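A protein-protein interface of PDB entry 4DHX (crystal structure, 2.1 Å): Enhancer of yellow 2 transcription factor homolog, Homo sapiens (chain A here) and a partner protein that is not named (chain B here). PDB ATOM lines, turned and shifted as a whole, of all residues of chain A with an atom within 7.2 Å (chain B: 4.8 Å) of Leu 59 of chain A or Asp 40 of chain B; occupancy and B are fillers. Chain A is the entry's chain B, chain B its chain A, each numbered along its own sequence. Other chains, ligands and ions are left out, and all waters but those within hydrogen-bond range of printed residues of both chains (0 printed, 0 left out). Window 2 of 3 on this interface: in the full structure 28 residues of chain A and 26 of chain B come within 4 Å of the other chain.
OE2 of Glu 60 of chain A is in salt-bridge range of NH2 of Arg 44 of chain B (3.1 Å).
Among the printed residues, pairs that only touch across the chains: Leu 59 of chain A with Leu 33 of chain B (3.5 Å), Leu 59 of chain A with Asp 40 of chain B (3.7 Å), Leu 59 of chain A with Ala 36 of chain B (3.9 Å), Thr 63 of chain A with Leu 33 of chain B (3.9 Å) and Val 62 of chain A with Leu 33 of chain B (3.9 Å).
Hydrophobic or aromatic side chains of chain A within 4 Å of the printed part of chain B: Leu 59 and Val 62. Printed residues of chain B that touch a printed residue of chain A: Leu 33, Ala 36, Asp 40 and Arg 44. Among the printed residues, 6 pairs touch across the chains.
The guanidinium group of Arg 44 of chain B is in salt-bridge range of the side-chain carboxylate of Asp 40 of chain B (2.9 Å).
Of chain B, only Leu 33 (3.5 Å), Ala 36 (3.9 Å) and Asp 40 (3.7 Å) come within 4 Å of Leu 59 of chain A. Of the printed residues of chain A, Asp 40 of chain B touches Leu 59. Printed residues of chain A within 4 Å of Ala 36 of chain B: Leu 59 (3.9 Å). Of the printed residues of chain A, Arg 44 of chain B touches Glu 60. Of the printed residues of chain B, Glu 60 of chain A touches Arg 44 (3.1 Å). Printed residues of chain B within 4 Å of Thr 63 of chain A: Leu 33. Printed residues of chain B within 4 Å of Val 62 of chain A: Leu 33 (3.9 Å). Lys 57 of chain A touches none of the printed residues of chain B. Gly 58 of chain A touches none of the printed residues of chain B. The nearest residue of chain A that does not touch Asp 40 of chain B is Glu 60 of chain A (6.2 Å).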
ATOM      1  N   VAL A  53      19.995  -2.435  14.873  1.00  0.00           N
ATOM      2  CA  VAL A  53      19.885  -0.980  14.935  1.00  0.00           C
ATOM      3  C   VAL A  53      20.899  -0.318  14.005  1.00  0.00           C
ATOM      4  O   VAL A  53      20.600   0.692  13.368  1.00  0.00           O
ATOM      5  CB  VAL A  53      20.078  -0.450  16.366  1.00  0.00           C
ATOM      6  CG1 VAL A  53      20.188   1.070  16.364  1.00  0.00           C
ATOM      7  CG2 VAL A  53      18.924  -0.896  17.252  1.00  0.00           C
ATOM      8  N   ILE A  54      22.095  -0.890  13.929  1.00  0.00           N
ATOM      9  CA  ILE A  54      23.119  -0.389  13.025  1.00  0.00           C
ATOM     10  C   ILE A  54      22.645  -0.509  11.579  1.00  0.00           C
ATOM     11  O   ILE A  54      22.744   0.439  10.802  1.00  0.00           O
ATOM     12  CB  ILE A  54      24.446  -1.154  13.196  1.00  0.00           C
ATOM     13  CG1 ILE A  54      25.139  -0.718  14.489  1.00  0.00           C
ATOM     14  CG2 ILE A  54      25.361  -0.906  12.002  1.00  0.00           C
ATOM     15  CD1 ILE A  54      26.418  -1.475  14.791  1.00  0.00           C
ATOM     16  N   LYS A  55      22.127  -1.682  11.230  1.00  0.00           N
ATOM     17  CA  LYS A  55      21.638  -1.935   9.881  1.00  0.00           C
ATOM     18  C   LYS A  55      20.459  -1.028   9.534  1.00  0.00           C
ATOM     19  O   LYS A  55      20.268  -0.663   8.375  1.00  0.00           O
ATOM     20  CB  LYS A  55      21.231  -3.404   9.740  1.00  0.00           C
ATOM     21  CG  LYS A  55      20.869  -3.815   8.324  1.00  0.00           C
ATOM     22  CD  LYS A  55      20.932  -5.329   8.142  1.00  0.00           C
ATOM     23  CE  LYS A  55      19.868  -6.053   8.953  1.00  0.00           C
ATOM     24  NZ  LYS A  55      18.493  -5.807   8.440  1.00  0.00           N
ATOM     25  N   GLU A  56      19.675  -0.661  10.543  1.00  0.00           N
ATOM     26  CA  GLU A  56      18.487   0.166  10.334  1.00  0.00           C
ATOM     27  C   GLU A  56      18.827   1.648  10.186  1.00  0.00           C
ATOM     28  O   GLU A  56      18.297   2.327   9.307  1.00  0.00           O
ATOM     29  CB  GLU A  56      17.508  -0.018  11.497  1.00  0.00           C
ATOM     30  CG  GLU A  56      16.824  -1.377  11.530  1.00  0.00           C
ATOM     31  CD  GLU A  56      15.688  -1.489  10.529  1.00  0.00           C
ATOM     32  OE1 GLU A  56      15.428  -0.507   9.803  1.00  0.00           O
ATOM     33  OE2 GLU A  56      15.055  -2.564  10.471  1.00  0.00           O
ATOM     34  N   LYS A  57      19.708   2.146  11.048  1.00  0.00           N
ATOM     35  CA  LYS A  57      20.025   3.570  11.081  1.00  0.00           C
ATOM     36  C   LYS A  57      21.156   3.927  10.119  1.00  0.00           C
ATOM     37  O   LYS A  57      21.127   4.975   9.472  1.00  0.00           O
ATOM     38  CB  LYS A  57      20.397   3.995  12.502  1.00  0.00           C
ATOM     39  CG  LYS A  57      19.300   3.757  13.531  1.00  0.00           C
ATOM     40  CD  LYS A  57      18.034   4.531  13.199  1.00  0.00           C
ATOM     41  CE  LYS A  57      16.980   4.362  14.282  1.00  0.00           C
ATOM     42  NZ  LYS A  57      15.743   5.139  13.991  1.00  0.00           N
ATOM     43  N   GLY A  58      22.153   3.052  10.035  1.00  0.00           N
ATOM     44  CA  GLY A  58      23.293   3.275   9.164  1.00  0.00           C
ATOM     45  C   GLY A  58      24.485   3.837   9.916  1.00  0.00           C
ATOM     46  O   GLY A  58      24.330   4.675  10.803  1.00  0.00           O
ATOM     47  N   LEU A  59      25.678   3.376   9.554  1.00  0.00           N
ATOM     48  CA  LEU A  59      26.908   3.824  10.202  1.00  0.00           C
ATOM     49  C   LEU A  59      27.190   5.297   9.934  1.00  0.00           C
ATOM     50  O   LEU A  59      27.898   5.951  10.700  1.00  0.00           O
ATOM     51  CB  LEU A  59      28.094   2.980   9.730  1.00  0.00           C
ATOM     52  CG  LEU A  59      28.106   1.529  10.214  1.00  0.00           C
ATOM     53  CD1 LEU A  59      29.166   0.730   9.476  1.00  0.00           C
ATOM     54  CD2 LEU A  59      28.337   1.469  11.718  1.00  0.00           C
ATOM     55  N   GLU A  60      26.638   5.819   8.846  1.00  0.00           N
ATOM     56  CA  GLU A  60      26.819   7.226   8.512  1.00  0.00           C
ATOM     57  C   GLU A  60      25.965   8.130   9.402  1.00  0.00           C
ATOM     58  O   GLU A  60      26.074   9.354   9.335  1.00  0.00           O
ATOM     59  CB  GLU A  60      26.484   7.468   7.038  1.00  0.00           C
ATOM     60  CG  GLU A  60      27.447   6.789   6.073  1.00  0.00           C
ATOM     61  CD  GLU A  60      27.121   7.077   4.619  1.00  0.00           C
ATOM     62  OE1 GLU A  60      26.028   7.618   4.346  1.00  0.00           O
ATOM     63  OE2 GLU A  60      27.960   6.766   3.747  1.00  0.00           O
ATOM     64  N   HIS A  61      25.124   7.526  10.239  1.00  0.00           N
ATOM     65  CA  HIS A  61      24.210   8.289  11.085  1.00  0.00           C
ATOM     66  C   HIS A  61      24.259   7.906  12.565  1.00  0.00           C
ATOM     67  O   HIS A  61      24.174   8.774  13.433  1.00  0.00           O
ATOM     68  CB  HIS A  61      22.774   8.124  10.580  1.00  0.00           C
ATOM     69  CG  HIS A  61      22.574   8.587   9.171  1.00  0.00           C
ATOM     70  ND1 HIS A  61      22.604   9.918   8.813  1.00  0.00           N
ATOM     71  CD2 HIS A  61      22.339   7.897   8.030  1.00  0.00           C
ATOM     72  CE1 HIS A  61      22.396  10.027   7.512  1.00  0.00           C
ATOM     73  NE2 HIS A  61      22.232   8.815   7.014  1.00  0.00           N
ATOM     74  N   VAL A  62      24.387   6.615  12.854  1.00  0.00           N
ATOM     75  CA  VAL A  62      24.237   6.128  14.223  1.00  0.00           C
ATOM     76  C   VAL A  62      25.452   6.440  15.094  1.00  0.00           C
ATOM     77  O   VAL A  62      26.595   6.381  14.639  1.00  0.00           O
ATOM     78  CB  VAL A  62      23.974   4.603  14.254  1.00  0.00           C
ATOM     79  CG1 VAL A  62      25.253   3.833  13.974  1.00  0.00           C
ATOM     80  CG2 VAL A  62      23.380   4.190  15.591  1.00  0.00           C
ATOM     81  N   THR A  63      25.186   6.784  16.350  1.00  0.00           N
ATOM     82  CA  THR A  63      26.234   6.990  17.341  1.00  0.00           C
ATOM     83  C   THR A  63      26.047   6.017  18.501  1.00  0.00           C
ATOM     84  O   THR A  63      25.046   5.304  18.567  1.00  0.00           O
ATOM     85  CB  THR A  63      26.212   8.426  17.894  1.00  0.00           C
ATOM     86  OG1 THR A  63      24.973   8.662  18.572  1.00  0.00           O
ATOM     87  CG2 THR A  63      26.373   9.438  16.768  1.00  0.00           C
ATOM     88  N   LEU B  33      29.861  -1.095  17.813  1.00  0.00           N
ATOM     89  CA  LEU B  33      29.960  -0.028  16.826  1.00  0.00           C
ATOM     90  C   LEU B  33      31.401   0.144  16.363  1.00  0.00           C
ATOM     91  O   LEU B  33      31.656   0.414  15.191  1.00  0.00           O
ATOM     92  CB  LEU B  33      29.430   1.287  17.395  1.00  0.00           C
ATOM     93  CG  LEU B  33      29.400   2.463  16.415  1.00  0.00           C
ATOM     94  CD1 LEU B  33      28.585   2.113  15.174  1.00  0.00           C
ATOM     95  CD2 LEU B  33      28.841   3.705  17.086  1.00  0.00           C
ATOM     96  N   ALA B  36      32.086  -2.596  13.867  1.00  0.00           N
ATOM     97  CA  ALA B  36      31.379  -2.306  12.625  1.00  0.00           C
ATOM     98  C   ALA B  36      32.099  -1.226  11.822  1.00  0.00           C
ATOM     99  O   ALA B  36      32.248  -1.346  10.604  1.00  0.00           O
ATOM    100  CB  ALA B  36      29.947  -1.879  12.924  1.00  0.00           C
ATOM    101  N   VAL B  37      32.544  -0.173  12.501  1.00  0.00           N
ATOM    102  CA  VAL B  37      33.227   0.930  11.833  1.00  0.00           C
ATOM    103  C   VAL B  37      34.582   0.484  11.283  1.00  0.00           C
ATOM    104  O   VAL B  37      35.000   0.919  10.208  1.00  0.00           O
ATOM    105  CB  VAL B  37      33.422   2.131  12.781  1.00  0.00           C
ATOM    106  CG1 VAL B  37      34.342   3.169  12.154  1.00  0.00           C
ATOM    107  CG2 VAL B  37      32.078   2.754  13.124  1.00  0.00           C
ATOM    108  N   GLU B  38      35.258  -0.388  12.024  1.00  0.00           N
ATOM    109  CA  GLU B  38      36.545  -0.926  11.599  1.00  0.00           C
ATOM    110  C   GLU B  38      36.377  -1.781  10.346  1.00  0.00           C
ATOM    111  O   GLU B  38      37.161  -1.680   9.401  1.00  0.00           O
ATOM    112  CB  GLU B  38      37.158  -1.767  12.717  1.00  0.00           C
ATOM    113  CG  GLU B  38      38.499  -2.385  12.368  1.00  0.00           C
ATOM    114  CD  GLU B  38      39.015  -3.306  13.457  1.00  0.00           C
ATOM    115  OE1 GLU B  38      38.270  -3.558  14.427  1.00  0.00           O
ATOM    116  OE2 GLU B  38      40.166  -3.777  13.346  1.00  0.00           O
ATOM    117  N   THR B  39      35.352  -2.626  10.351  1.00  0.00           N
ATOM    118  CA  THR B  39      35.056  -3.481   9.206  1.00  0.00           C
ATOM    119  C   THR B  39      34.676  -2.636   7.994  1.00  0.00           C
ATOM    120  O   THR B  39      35.153  -2.874   6.885  1.00  0.00           O
ATOM    121  CB  THR B  39      33.912  -4.461   9.520  1.00  0.00           C
ATOM    122  OG1 THR B  39      34.318  -5.357  10.562  1.00  0.00           O
ATOM    123  CG2 THR B  39      33.538  -5.271   8.283  1.00  0.00           C
ATOM    124  N   ASP B  40      33.819  -1.646   8.213  1.00  0.00           N
ATOM    125  CA  ASP B  40      33.380  -0.766   7.141  1.00  0.00           C
ATOM    126  C   ASP B  40      34.561  -0.007   6.549  1.00  0.00           C
ATOM    127  O   ASP B  40      34.603   0.257   5.346  1.00  0.00           O
ATOM    128  CB  ASP B  40      32.339   0.224   7.655  1.00  0.00           C
ATOM    129  CG  ASP B  40      31.784   1.103   6.553  1.00  0.00           C
ATOM    130  OD1 ASP B  40      31.358   0.552   5.518  1.00  0.00           O
ATOM    131  OD2 ASP B  40      31.787   2.342   6.713  1.00  0.00           O
ATOM    132  N   GLN B  41      35.517   0.349   7.399  1.00  0.00           N
ATOM    133  CA  GLN B  41      36.710   1.052   6.948  1.00  0.00           C
ATOM    134  C   GLN B  41      37.474   0.189   5.945  1.00  0.00           C
ATOM    135  O   GLN B  41      37.919   0.680   4.909  1.00  0.00           O
ATOM    136  CB  GLN B  41      37.603   1.413   8.139  1.00  0.00           C
ATOM    137  CG  GLN B  41      38.863   2.186   7.770  1.00  0.00           C
ATOM    138  CD  GLN B  41      38.572   3.591   7.274  1.00  0.00           C
ATOM    139  OE1 GLN B  41      37.418   4.021   7.226  1.00  0.00           O
ATOM    140  NE2 GLN B  41      39.621   4.314   6.900  1.00  0.00           N
ATOM    141  N   ARG B  42      37.614  -1.098   6.251  1.00  0.00           N
ATOM    142  CA  ARG B  42      38.283  -2.027   5.349  1.00  0.00           C
ATOM    143  C   ARG B  42      37.514  -2.133   4.036  1.00  0.00           C
ATOM    144  O   ARG B  42      38.109  -2.228   2.963  1.00  0.00           O
ATOM    145  CB  ARG B  42      38.410  -3.413   5.987  1.00  0.00           C
ATOM    146  CG  ARG B  42      39.301  -3.458   7.216  1.00  0.00           C
ATOM    147  CD  ARG B  42      39.663  -4.891   7.589  1.00  0.00           C
ATOM    148  NE  ARG B  42      38.499  -5.677   7.995  1.00  0.00           N
ATOM    149  CZ  ARG B  42      38.026  -5.750   9.237  1.00  0.00           C
ATOM    150  NH1 ARG B  42      38.601  -5.082  10.229  1.00  0.00           N
ATOM    151  NH2 ARG B  42      36.962  -6.499   9.486  1.00  0.00           N
ATOM    152  N   VAL B  43      36.189  -2.121   4.130  1.00  0.00           N
ATOM    153  CA  VAL B  43      35.339  -2.175   2.949  1.00  0.00           C
ATOM    154  C   VAL B  43      35.574  -0.950   2.070  1.00  0.00           C
ATOM    155  O   VAL B  43      35.732  -1.067   0.856  1.00  0.00           O
ATOM    156  CB  VAL B  43      33.846  -2.244   3.328  1.00  0.00           C
ATOM    157  CG1 VAL B  43      32.969  -2.060   2.096  1.00  0.00           C
ATOM    158  CG2 VAL B  43      33.528  -3.565   4.016  1.00  0.00           C
ATOM    159  N   ARG B  44      35.605   0.226   2.690  1.00  0.00           N
ATOM    160  CA  ARG B  44      35.768   1.472   1.950  1.00  0.00           C
ATOM    161  C   ARG B  44      37.146   1.586   1.306  1.00  0.00           C
ATOM    162  O   ARG B  44      37.276   2.120   0.207  1.00  0.00           O
ATOM    163  CB  ARG B  44      35.526   2.676   2.860  1.00  0.00           C
ATOM    164  CG  ARG B  44      34.088   2.831   3.321  1.00  0.00           C
ATOM    165  CD  ARG B  44      33.922   4.064   4.199  1.00  0.00           C
ATOM    166  NE  ARG B  44      32.536   4.262   4.612  1.00  0.00           N
ATOM    167  CZ  ARG B  44      31.595   4.817   3.853  1.00  0.00           C
ATOM    168  NH1 ARG B  44      31.875   5.231   2.624  1.00  0.00           N
ATOM    169  NH2 ARG B  44      30.363   4.954   4.321  1.00  0.00           N
